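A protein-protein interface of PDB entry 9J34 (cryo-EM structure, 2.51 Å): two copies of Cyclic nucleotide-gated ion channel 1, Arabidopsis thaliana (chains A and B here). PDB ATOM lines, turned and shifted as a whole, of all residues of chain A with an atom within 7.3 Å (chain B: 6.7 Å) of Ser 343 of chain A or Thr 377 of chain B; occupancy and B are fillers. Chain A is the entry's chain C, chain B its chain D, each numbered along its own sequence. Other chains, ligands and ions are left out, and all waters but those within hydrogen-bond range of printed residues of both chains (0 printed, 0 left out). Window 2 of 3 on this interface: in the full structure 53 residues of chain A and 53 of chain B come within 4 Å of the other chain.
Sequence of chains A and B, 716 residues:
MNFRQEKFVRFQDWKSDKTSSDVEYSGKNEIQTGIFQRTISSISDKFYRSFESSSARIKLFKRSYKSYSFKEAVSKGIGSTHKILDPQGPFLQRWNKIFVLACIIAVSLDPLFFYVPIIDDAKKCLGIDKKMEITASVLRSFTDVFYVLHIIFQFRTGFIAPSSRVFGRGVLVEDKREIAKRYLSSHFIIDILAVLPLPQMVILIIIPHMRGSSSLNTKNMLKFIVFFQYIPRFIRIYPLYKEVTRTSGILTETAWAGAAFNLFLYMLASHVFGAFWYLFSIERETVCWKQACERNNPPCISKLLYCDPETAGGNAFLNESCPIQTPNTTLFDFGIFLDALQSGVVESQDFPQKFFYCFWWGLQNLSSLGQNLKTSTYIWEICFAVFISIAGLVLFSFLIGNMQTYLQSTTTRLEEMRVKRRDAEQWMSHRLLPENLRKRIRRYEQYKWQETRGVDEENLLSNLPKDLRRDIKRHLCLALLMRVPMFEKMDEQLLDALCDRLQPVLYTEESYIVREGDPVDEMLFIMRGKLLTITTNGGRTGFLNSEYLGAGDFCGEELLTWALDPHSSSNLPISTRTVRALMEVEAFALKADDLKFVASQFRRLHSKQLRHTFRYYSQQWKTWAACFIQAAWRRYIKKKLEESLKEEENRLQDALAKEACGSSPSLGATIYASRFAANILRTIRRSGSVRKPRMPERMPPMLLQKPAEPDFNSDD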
ATOM      1  N   TRP A 277      26.217  11.806  21.418  1.00  0.00           N
ATOM      2  CA  TRP A 277      25.280  11.149  20.518  1.00  0.00           C
ATOM      3  C   TRP A 277      23.917  11.816  20.534  1.00  0.00           C
ATOM      4  O   TRP A 277      23.243  11.852  19.504  1.00  0.00           O
ATOM      5  CB  TRP A 277      25.150   9.687  20.912  1.00  0.00           C
ATOM      6  CG  TRP A 277      24.123   8.909  20.165  1.00  0.00           C
ATOM      7  CD1 TRP A 277      24.168   8.538  18.858  1.00  0.00           C
ATOM      8  CD2 TRP A 277      22.906   8.378  20.689  1.00  0.00           C
ATOM      9  NE1 TRP A 277      23.057   7.815  18.533  1.00  0.00           N
ATOM     10  CE2 TRP A 277      22.261   7.702  19.639  1.00  0.00           C
ATOM     11  CE3 TRP A 277      22.294   8.412  21.946  1.00  0.00           C
ATOM     12  CZ2 TRP A 277      21.042   7.057  19.806  1.00  0.00           C
ATOM     13  CZ3 TRP A 277      21.081   7.778  22.108  1.00  0.00           C
ATOM     14  CH2 TRP A 277      20.470   7.106  21.046  1.00  0.00           C
ATOM     15  N   ILE A 324      11.339   9.490   9.814  1.00  0.00           N
ATOM     16  CA  ILE A 324      11.979   8.981  11.021  1.00  0.00           C
ATOM     17  C   ILE A 324      11.287   7.724  11.535  1.00  0.00           C
ATOM     18  O   ILE A 324      11.933   6.692  11.747  1.00  0.00           O
ATOM     19  CB  ILE A 324      12.040  10.064  12.123  1.00  0.00           C
ATOM     20  CG1 ILE A 324      13.072  11.124  11.756  1.00  0.00           C
ATOM     21  CG2 ILE A 324      12.390   9.465  13.472  1.00  0.00           C
ATOM     22  CD1 ILE A 324      13.040  12.315  12.647  1.00  0.00           C
ATOM     23  N   GLN A 325       9.966   7.789  11.736  1.00  0.00           N
ATOM     24  CA  GLN A 325       9.250   6.664  12.328  1.00  0.00           C
ATOM     25  C   GLN A 325       9.134   5.498  11.359  1.00  0.00           C
ATOM     26  O   GLN A 325       9.178   4.336  11.781  1.00  0.00           O
ATOM     27  CB  GLN A 325       7.872   7.114  12.803  1.00  0.00           C
ATOM     28  CG  GLN A 325       7.919   8.142  13.926  1.00  0.00           C
ATOM     29  CD  GLN A 325       8.630   7.635  15.174  1.00  0.00           C
ATOM     30  OE1 GLN A 325       8.540   6.458  15.527  1.00  0.00           O
ATOM     31  NE2 GLN A 325       9.337   8.530  15.850  1.00  0.00           N
ATOM     32  N   PHE A 337      22.018   7.640  14.536  1.00  0.00           N
ATOM     33  CA  PHE A 337      21.217   8.634  15.227  1.00  0.00           C
ATOM     34  C   PHE A 337      19.728   8.370  15.119  1.00  0.00           C
ATOM     35  O   PHE A 337      18.947   9.099  15.731  1.00  0.00           O
ATOM     36  CB  PHE A 337      21.527  10.028  14.681  1.00  0.00           C
ATOM     37  CG  PHE A 337      22.985  10.330  14.609  1.00  0.00           C
ATOM     38  CD1 PHE A 337      23.740  10.413  15.761  1.00  0.00           C
ATOM     39  CD2 PHE A 337      23.607  10.515  13.389  1.00  0.00           C
ATOM     40  CE1 PHE A 337      25.080  10.680  15.700  1.00  0.00           C
ATOM     41  CE2 PHE A 337      24.951  10.791  13.323  1.00  0.00           C
ATOM     42  CZ  PHE A 337      25.688  10.873  14.479  1.00  0.00           C
ATOM     43  N   LEU A 338      19.323   7.353  14.356  1.00  0.00           N
ATOM     44  CA  LEU A 338      17.907   7.073  14.151  1.00  0.00           C
ATOM     45  C   LEU A 338      17.233   6.581  15.425  1.00  0.00           C
ATOM     46  O   LEU A 338      16.047   6.850  15.635  1.00  0.00           O
ATOM     47  CB  LEU A 338      17.741   6.050  13.026  1.00  0.00           C
ATOM     48  CG  LEU A 338      16.326   5.669  12.585  1.00  0.00           C
ATOM     49  CD1 LEU A 338      15.660   6.819  11.861  1.00  0.00           C
ATOM     50  CD2 LEU A 338      16.350   4.433  11.722  1.00  0.00           C
ATOM     51  N   ASP A 339      17.975   5.883  16.290  1.00  0.00           N
ATOM     52  CA  ASP A 339      17.407   5.389  17.540  1.00  0.00           C
ATOM     53  C   ASP A 339      17.062   6.530  18.491  1.00  0.00           C
ATOM     54  O   ASP A 339      16.101   6.431  19.259  1.00  0.00           O
ATOM     55  CB  ASP A 339      18.376   4.416  18.205  1.00  0.00           C
ATOM     56  CG  ASP A 339      18.170   2.990  17.748  1.00  0.00           C
ATOM     57  OD1 ASP A 339      17.093   2.693  17.187  1.00  0.00           O
ATOM     58  OD2 ASP A 339      19.087   2.166  17.938  1.00  0.00           O
ATOM     59  N   ALA A 340      17.830   7.620  18.454  1.00  0.00           N
ATOM     60  CA  ALA A 340      17.513   8.771  19.291  1.00  0.00           C
ATOM     61  C   ALA A 340      16.302   9.528  18.779  1.00  0.00           C
ATOM     62  O   ALA A 340      15.539  10.081  19.575  1.00  0.00           O
ATOM     63  CB  ALA A 340      18.703   9.719  19.369  1.00  0.00           C
ATOM     64  N   LEU A 341      16.115   9.579  17.464  1.00  0.00           N
ATOM     65  CA  LEU A 341      14.997  10.327  16.913  1.00  0.00           C
ATOM     66  C   LEU A 341      13.711   9.516  16.930  1.00  0.00           C
ATOM     67  O   LEU A 341      12.620  10.095  16.918  1.00  0.00           O
ATOM     68  CB  LEU A 341      15.321  10.786  15.492  1.00  0.00           C
ATOM     69  CG  LEU A 341      16.676  11.462  15.279  1.00  0.00           C
ATOM     70  CD1 LEU A 341      16.839  11.871  13.834  1.00  0.00           C
ATOM     71  CD2 LEU A 341      16.869  12.653  16.200  1.00  0.00           C
ATOM     72  N   GLN A 342      13.814   8.188  16.964  1.00  0.00           N
ATOM     73  CA  GLN A 342      12.627   7.345  17.007  1.00  0.00           C
ATOM     74  C   GLN A 342      12.118   7.143  18.426  1.00  0.00           C
ATOM     75  O   GLN A 342      10.909   6.997  18.627  1.00  0.00           O
ATOM     76  CB  GLN A 342      12.921   5.989  16.369  1.00  0.00           C
ATOM     77  CG  GLN A 342      12.866   5.994  14.864  1.00  0.00           C
ATOM     78  CD  GLN A 342      13.191   4.646  14.267  1.00  0.00           C
ATOM     79  OE1 GLN A 342      13.828   3.812  14.903  1.00  0.00           O
ATOM     80  NE2 GLN A 342      12.748   4.423  13.039  1.00  0.00           N
ATOM     81  N   SER A 343      13.011   7.128  19.412  1.00  0.00           N
ATOM     82  CA  SER A 343      12.608   6.962  20.799  1.00  0.00           C
ATOM     83  C   SER A 343      11.997   8.220  21.396  1.00  0.00           C
ATOM     84  O   SER A 343      11.396   8.144  22.473  1.00  0.00           O
ATOM     85  CB  SER A 343      13.804   6.536  21.648  1.00  0.00           C
ATOM     86  OG  SER A 343      14.788   7.547  21.671  1.00  0.00           O
ATOM     87  N   GLY A 344      12.131   9.365  20.733  1.00  0.00           N
ATOM     88  CA  GLY A 344      11.613  10.599  21.274  1.00  0.00           C
ATOM     89  C   GLY A 344      12.406  11.160  22.426  1.00  0.00           C
ATOM     90  O   GLY A 344      11.889  11.994  23.170  1.00  0.00           O
ATOM     91  N   VAL A 345      13.654  10.722  22.601  1.00  0.00           N
ATOM     92  CA  VAL A 345      14.492  11.252  23.668  1.00  0.00           C
ATOM     93  C   VAL A 345      14.946  12.674  23.356  1.00  0.00           C
ATOM     94  O   VAL A 345      15.224  13.448  24.279  1.00  0.00           O
ATOM     95  CB  VAL A 345      15.676  10.293  23.918  1.00  0.00           C
ATOM     96  CG1 VAL A 345      16.687  10.309  22.774  1.00  0.00           C
ATOM     97  CG2 VAL A 345      16.343  10.562  25.247  1.00  0.00           C
ATOM     98  N   VAL A 346      14.965  13.061  22.079  1.00  0.00           N
ATOM     99  CA  VAL A 346      15.338  14.419  21.698  1.00  0.00           C
ATOM    100  C   VAL A 346      14.189  15.401  21.843  1.00  0.00           C
ATOM    101  O   VAL A 346      14.391  16.606  21.658  1.00  0.00           O
ATOM    102  CB  VAL A 346      15.870  14.427  20.253  1.00  0.00           C
ATOM    103  CG1 VAL A 346      17.121  13.579  20.151  1.00  0.00           C
ATOM    104  CG2 VAL A 346      14.810  13.924  19.297  1.00  0.00           C
ATOM    105  N   GLU A 347      12.990  14.920  22.169  1.00  0.00           N
ATOM    106  CA  GLU A 347      11.838  15.773  22.420  1.00  0.00           C
ATOM    107  C   GLU A 347      11.468  15.860  23.888  1.00  0.00           C
ATOM    108  O   GLU A 347      10.746  16.785  24.275  1.00  0.00           O
ATOM    109  CB  GLU A 347      10.620  15.270  21.642  1.00  0.00           C
ATOM    110  CG  GLU A 347      10.926  14.823  20.233  1.00  0.00           C
ATOM    111  CD  GLU A 347       9.885  13.876  19.697  1.00  0.00           C
ATOM    112  OE1 GLU A 347       8.767  13.850  20.247  1.00  0.00           O
ATOM    113  OE2 GLU A 347      10.188  13.148  18.730  1.00  0.00           O
ATOM    114  N   SER A 348      11.929  14.918  24.700  1.00  0.00           N
ATOM    115  CA  SER A 348      11.554  14.872  26.102  1.00  0.00           C
ATOM    116  C   SER A 348      12.255  15.973  26.880  1.00  0.00           C
ATOM    117  O   SER A 348      13.424  16.267  26.644  1.00  0.00           O
ATOM    118  CB  SER A 348      11.915  13.508  26.687  1.00  0.00           C
ATOM    119  OG  SER A 348      11.953  13.546  28.099  1.00  0.00           O
ATOM    120  N   PRO A 352      15.936  12.675  33.833  1.00  0.00           N
ATOM    121  CA  PRO A 352      16.371  11.286  34.077  1.00  0.00           C
ATOM    122  C   PRO A 352      15.930  10.319  32.995  1.00  0.00           C
ATOM    123  O   PRO A 352      16.597   9.303  32.780  1.00  0.00           O
ATOM    124  CB  PRO A 352      15.734  10.943  35.431  1.00  0.00           C
ATOM    125  CG  PRO A 352      15.490  12.236  36.060  1.00  0.00           C
ATOM    126  CD  PRO A 352      15.067  13.115  34.945  1.00  0.00           C
ATOM    127  N   GLN A 353      14.829  10.614  32.308  1.00  0.00           N
ATOM    128  CA  GLN A 353      14.482   9.889  31.092  1.00  0.00           C
ATOM    129  C   GLN A 353      15.537  10.104  30.016  1.00  0.00           C
ATOM    130  O   GLN A 353      16.008   9.153  29.385  1.00  0.00           O
ATOM    131  CB  GLN A 353      13.108  10.349  30.608  1.00  0.00           C
ATOM    132  CG  GLN A 353      12.792  10.014  29.172  1.00  0.00           C
ATOM    133  CD  GLN A 353      12.697   8.532  28.947  1.00  0.00           C
ATOM    134  OE1 GLN A 353      13.600   7.922  28.378  1.00  0.00           O
ATOM    135  NE2 GLN A 353      11.606   7.932  29.405  1.00  0.00           N
ATOM    136  N   LYS A 354      15.947  11.356  29.824  1.00  0.00           N
ATOM    137  CA  LYS A 354      16.882  11.696  28.760  1.00  0.00           C
ATOM    138  C   LYS A 354      18.302  11.260  29.098  1.00  0.00           C
ATOM    139  O   LYS A 354      19.040  10.810  28.215  1.00  0.00           O
ATOM    140  CB  LYS A 354      16.818  13.198  28.507  1.00  0.00           C
ATOM    141  CG  LYS A 354      17.593  13.680  27.325  1.00  0.00           C
ATOM    142  CD  LYS A 354      17.787  15.166  27.424  1.00  0.00           C
ATOM    143  CE  LYS A 354      16.537  15.901  27.109  1.00  0.00           C
ATOM    144  NZ  LYS A 354      16.653  17.366  27.332  1.00  0.00           N
ATOM    145  N   PHE A 356      19.332   8.723  31.164  1.00  0.00           N
ATOM    146  CA  PHE A 356      19.556   7.286  31.276  1.00  0.00           C
ATOM    147  C   PHE A 356      19.516   6.595  29.924  1.00  0.00           C
ATOM    148  O   PHE A 356      20.247   5.625  29.715  1.00  0.00           O
ATOM    149  CB  PHE A 356      18.532   6.665  32.224  1.00  0.00           C
ATOM    150  CG  PHE A 356      18.988   6.620  33.648  1.00  0.00           C
ATOM    151  CD1 PHE A 356      20.005   5.766  34.031  1.00  0.00           C
ATOM    152  CD2 PHE A 356      18.411   7.442  34.603  1.00  0.00           C
ATOM    153  CE1 PHE A 356      20.437   5.729  35.341  1.00  0.00           C
ATOM    154  CE2 PHE A 356      18.835   7.409  35.914  1.00  0.00           C
ATOM    155  CZ  PHE A 356      19.848   6.552  36.284  1.00  0.00           C
ATOM    156  N   TYR A 357      18.681   7.075  29.002  1.00  0.00           N
ATOM    157  CA  TYR A 357      18.643   6.502  27.662  1.00  0.00           C
ATOM    158  C   TYR A 357      19.936   6.774  26.905  1.00  0.00           C
ATOM    159  O   TYR A 357      20.407   5.921  26.147  1.00  0.00           O
ATOM    160  CB  TYR A 357      17.447   7.055  26.891  1.00  0.00           C
ATOM    161  CG  TYR A 357      17.214   6.377  25.563  1.00  0.00           C
ATOM    162  CD1 TYR A 357      17.654   6.957  24.381  1.00  0.00           C
ATOM    163  CD2 TYR A 357      16.558   5.157  25.493  1.00  0.00           C
ATOM    164  CE1 TYR A 357      17.448   6.340  23.167  1.00  0.00           C
ATOM    165  CE2 TYR A 357      16.347   4.533  24.282  1.00  0.00           C
ATOM    166  CZ  TYR A 357      16.794   5.130  23.124  1.00  0.00           C
ATOM    167  OH  TYR A 357      16.587   4.514  21.914  1.00  0.00           O
ATOM    168  N   ASP B 333       5.813  -0.088  24.807  1.00  0.00           N
ATOM    169  CA  ASP B 333       7.108  -0.664  24.468  1.00  0.00           C
ATOM    170  C   ASP B 333       7.539  -1.566  25.617  1.00  0.00           C
ATOM    171  O   ASP B 333       7.798  -1.090  26.726  1.00  0.00           O
ATOM    172  CB  ASP B 333       8.138   0.430  24.208  1.00  0.00           C
ATOM    173  CG  ASP B 333       9.350  -0.071  23.443  1.00  0.00           C
ATOM    174  OD1 ASP B 333       9.421  -1.278  23.140  1.00  0.00           O
ATOM    175  OD2 ASP B 333      10.242   0.746  23.145  1.00  0.00           O
ATOM    176  N   THR B 375      16.571  -1.860  24.912  1.00  0.00           N
ATOM    177  CA  THR B 375      15.688  -1.342  25.941  1.00  0.00           C
ATOM    178  C   THR B 375      14.668  -0.375  25.351  1.00  0.00           C
ATOM    179  O   THR B 375      14.820   0.143  24.243  1.00  0.00           O
ATOM    180  CB  THR B 375      16.474  -0.618  27.035  1.00  0.00           C
ATOM    181  OG1 THR B 375      17.169   0.497  26.469  1.00  0.00           O
ATOM    182  CG2 THR B 375      17.465  -1.540  27.688  1.00  0.00           C
ATOM    183  N   SER B 376      13.617  -0.138  26.118  1.00  0.00           N
ATOM    184  CA  SER B 376      12.682   0.937  25.846  1.00  0.00           C
ATOM    185  C   SER B 376      13.197   2.208  26.518  1.00  0.00           C
ATOM    186  O   SER B 376      14.342   2.282  26.967  1.00  0.00           O
ATOM    187  CB  SER B 376      11.286   0.555  26.324  1.00  0.00           C
ATOM    188  OG  SER B 376      11.224   0.506  27.733  1.00  0.00           O
ATOM    189  N   THR B 377      12.354   3.226  26.599  1.00  0.00           N
ATOM    190  CA  THR B 377      12.713   4.458  27.282  1.00  0.00           C
ATOM    191  C   THR B 377      12.397   4.422  28.770  1.00  0.00           C
ATOM    192  O   THR B 377      12.560   5.439  29.447  1.00  0.00           O
ATOM    193  CB  THR B 377      12.001   5.643  26.629  1.00  0.00           C
ATOM    194  OG1 THR B 377      10.587   5.427  26.653  1.00  0.00           O
ATOM    195  CG2 THR B 377      12.460   5.807  25.195  1.00  0.00           C
ATOM    196  N   TYR B 378      11.953   3.281  29.288  1.00  0.00           N
ATOM    197  CA  TYR B 378      11.641   3.148  30.704  1.00  0.00           C
ATOM    198  C   TYR B 378      12.927   3.140  31.521  1.00  0.00           C
ATOM    199  O   TYR B 378      13.882   2.443  31.177  1.00  0.00           O
ATOM    200  CB  TYR B 378      10.834   1.871  30.926  1.00  0.00           C
ATOM    201  CG  TYR B 378      10.382   1.630  32.342  1.00  0.00           C
ATOM    202  CD1 TYR B 378      10.657   0.430  32.980  1.00  0.00           C
ATOM    203  CD2 TYR B 378       9.672   2.597  33.037  1.00  0.00           C
ATOM    204  CE1 TYR B 378      10.243   0.200  34.271  1.00  0.00           C
ATOM    205  CE2 TYR B 378       9.255   2.377  34.330  1.00  0.00           C
ATOM    206  CZ  TYR B 378       9.543   1.177  34.940  1.00  0.00           C
ATOM    207  OH  TYR B 378       9.128   0.950  36.227  1.00  0.00           O
ATOM    208  N   ILE B 379      12.941   3.914  32.611  1.00  0.00           N
ATOM    209  CA  ILE B 379      14.181   4.211  33.326  1.00  0.00           C
ATOM    210  C   ILE B 379      14.693   2.987  34.076  1.00  0.00           C
ATOM    211  O   ILE B 379      15.884   2.659  34.013  1.00  0.00           O
ATOM    212  CB  ILE B 379      13.969   5.415  34.266  1.00  0.00           C
ATOM    213  CG1 ILE B 379      14.021   6.722  33.482  1.00  0.00           C
ATOM    214  CG2 ILE B 379      15.006   5.466  35.380  1.00  0.00           C
ATOM    215  CD1 ILE B 379      13.678   7.928  34.320  1.00  0.00           C
ATOM    216  N   TRP B 380      13.810   2.278  34.779  1.00  0.00           N
ATOM    217  CA  TRP B 380      14.255   1.145  35.580  1.00  0.00           C
ATOM    218  C   TRP B 380      14.566  -0.078  34.738  1.00  0.00           C
ATOM    219  O   TRP B 380      15.306  -0.953  35.193  1.00  0.00           O
ATOM    220  CB  TRP B 380      13.214   0.818  36.648  1.00  0.00           C
ATOM    221  CG  TRP B 380      12.779   2.027  37.415  1.00  0.00           C
ATOM    222  CD1 TRP B 380      11.531   2.561  37.448  1.00  0.00           C
ATOM    223  CD2 TRP B 380      13.595   2.865  38.247  1.00  0.00           C
ATOM    224  NE1 TRP B 380      11.510   3.671  38.247  1.00  0.00           N
ATOM    225  CE2 TRP B 380      12.764   3.881  38.750  1.00  0.00           C
ATOM    226  CE3 TRP B 380      14.944   2.852  38.619  1.00  0.00           C
ATOM    227  CZ2 TRP B 380      13.235   4.874  39.603  1.00  0.00           C
ATOM    228  CZ3 TRP B 380      15.409   3.840  39.461  1.00  0.00           C
ATOM    229  CH2 TRP B 380      14.557   4.837  39.945  1.00  0.00           C
ATOM    230  N   GLU B 381      14.027  -0.149  33.523  1.00  0.00           N
ATOM    231  CA  GLU B 381      14.484  -1.149  32.568  1.00  0.00           C
ATOM    232  C   GLU B 381      15.902  -0.844  32.102  1.00  0.00           C
ATOM    233  O   GLU B 381      16.724  -1.756  31.947  1.00  0.00           O
ATOM    234  CB  GLU B 381      13.520  -1.204  31.389  1.00  0.00           C
ATOM    235  CG  GLU B 381      13.982  -2.081  30.265  1.00  0.00           C
ATOM    236  CD  GLU B 381      13.081  -2.020  29.073  1.00  0.00           C
ATOM    237  OE1 GLU B 381      13.435  -2.635  28.058  1.00  0.00           O
ATOM    238  OE2 GLU B 381      12.024  -1.366  29.146  1.00  0.00           O
ATOM    239  N   ILE B 382      16.207   0.439  31.893  1.00  0.00           N
ATOM    240  CA  ILE B 382      17.555   0.862  31.528  1.00  0.00           C
ATOM    241  C   ILE B 382      18.527   0.606  32.675  1.00  0.00           C
ATOM    242  O   ILE B 382      19.638   0.110  32.460  1.00  0.00           O
ATOM    243  CB  ILE B 382      17.535   2.344  31.105  1.00  0.00           C
ATOM    244  CG1 ILE B 382      16.862   2.511  29.747  1.00  0.00           C
ATOM    245  CG2 ILE B 382      18.919   2.935  31.066  1.00  0.00           C
ATOM    246  CD1 ILE B 382      16.487   3.930  29.437  1.00  0.00           C
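The backbone carbonyl oxygen (O) of Thr 377 of chain B is in hydrogen-bond range of the side-chain amide nitrogen (NE2) of Gln 353 of chain A.
Among the printed residues, 7 pairs touch across the chains.
OG of Ser 376 of chain B lies close to N of Tyr 378 of chain B (3.3 Å). OG of Ser 376 of chain B lies within hydrogen-bond range of OE2 of Glu 381 of chain B (2.5 Å). O of Asp 339 of chain A sits at hydrogen-bond distance from OG of Ser 343 of chain A (3.0 Å). The backbone carbonyl oxygen (O) of Asp 339 of chain A sits at hydrogen-bond distance from the side-chain hydroxyl (OH) of Tyr 357 of chain A (3.3 Å). The backbone carbonyl oxygen of Ala 340 of chain A lies within hydrogen-bond range of the side-chain hydroxyl of Ser 343 of chain A, 3.4 Å away. The side-chain hydroxyl of Ser 343 of chain A lies close to the backbone NH of Val 345 of chain A (3.5 Å).
No position is printed for both chains. Of the 7 pairs that touch across the chains among the printed residues, none has its exchanged pair printed and touching as well.
Of the printed residues of chain B, Ser 343 of chain A touches Thr 377 (3.7 Å). Of the printed residues of chain A, Thr 377 of chain B touches Ser 343 and Gln 353. Of the printed residues of chain B, Phe 356 of chain A touches Ile 382 (3.3 Å). Of the printed residues of chain A, Ile 379 of chain B touches Pro 352 and Gln 353. Printed residues of chain A within 4 Å of Ile 382 of chain B: Phe 356 (3.3 Å) and Tyr 357 (3.8 Å). Printed residues of chain B within 4 Å of Pro 352 of chain A: Ile 379 (3.5 Å). The nearest residue of chain B that does not touch Ser 343 of chain A is Ser 376 of chain B (6.5 Å). The nearest residue of chain A that does not touch Thr 377 of chain B is Tyr 357 of chain A (4.2 Å).
Thr 377 of chain B touches Ser 343 of chain A. C of Pro 352 of chain A touches CD1 of Ile 379 of chain B, 3.5 Å away. Ile 379 of chain B touches Gln 353 of chain A. O of Phe 356 of chain A touches CG2 of Ile 382 of chain B, 3.3 Å away. Ser 376 of chain B touches Tyr 357 of chain A. Ile 382 of chain B touches Tyr 357 of chain A (CD1 to CA, 3.8 Å).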
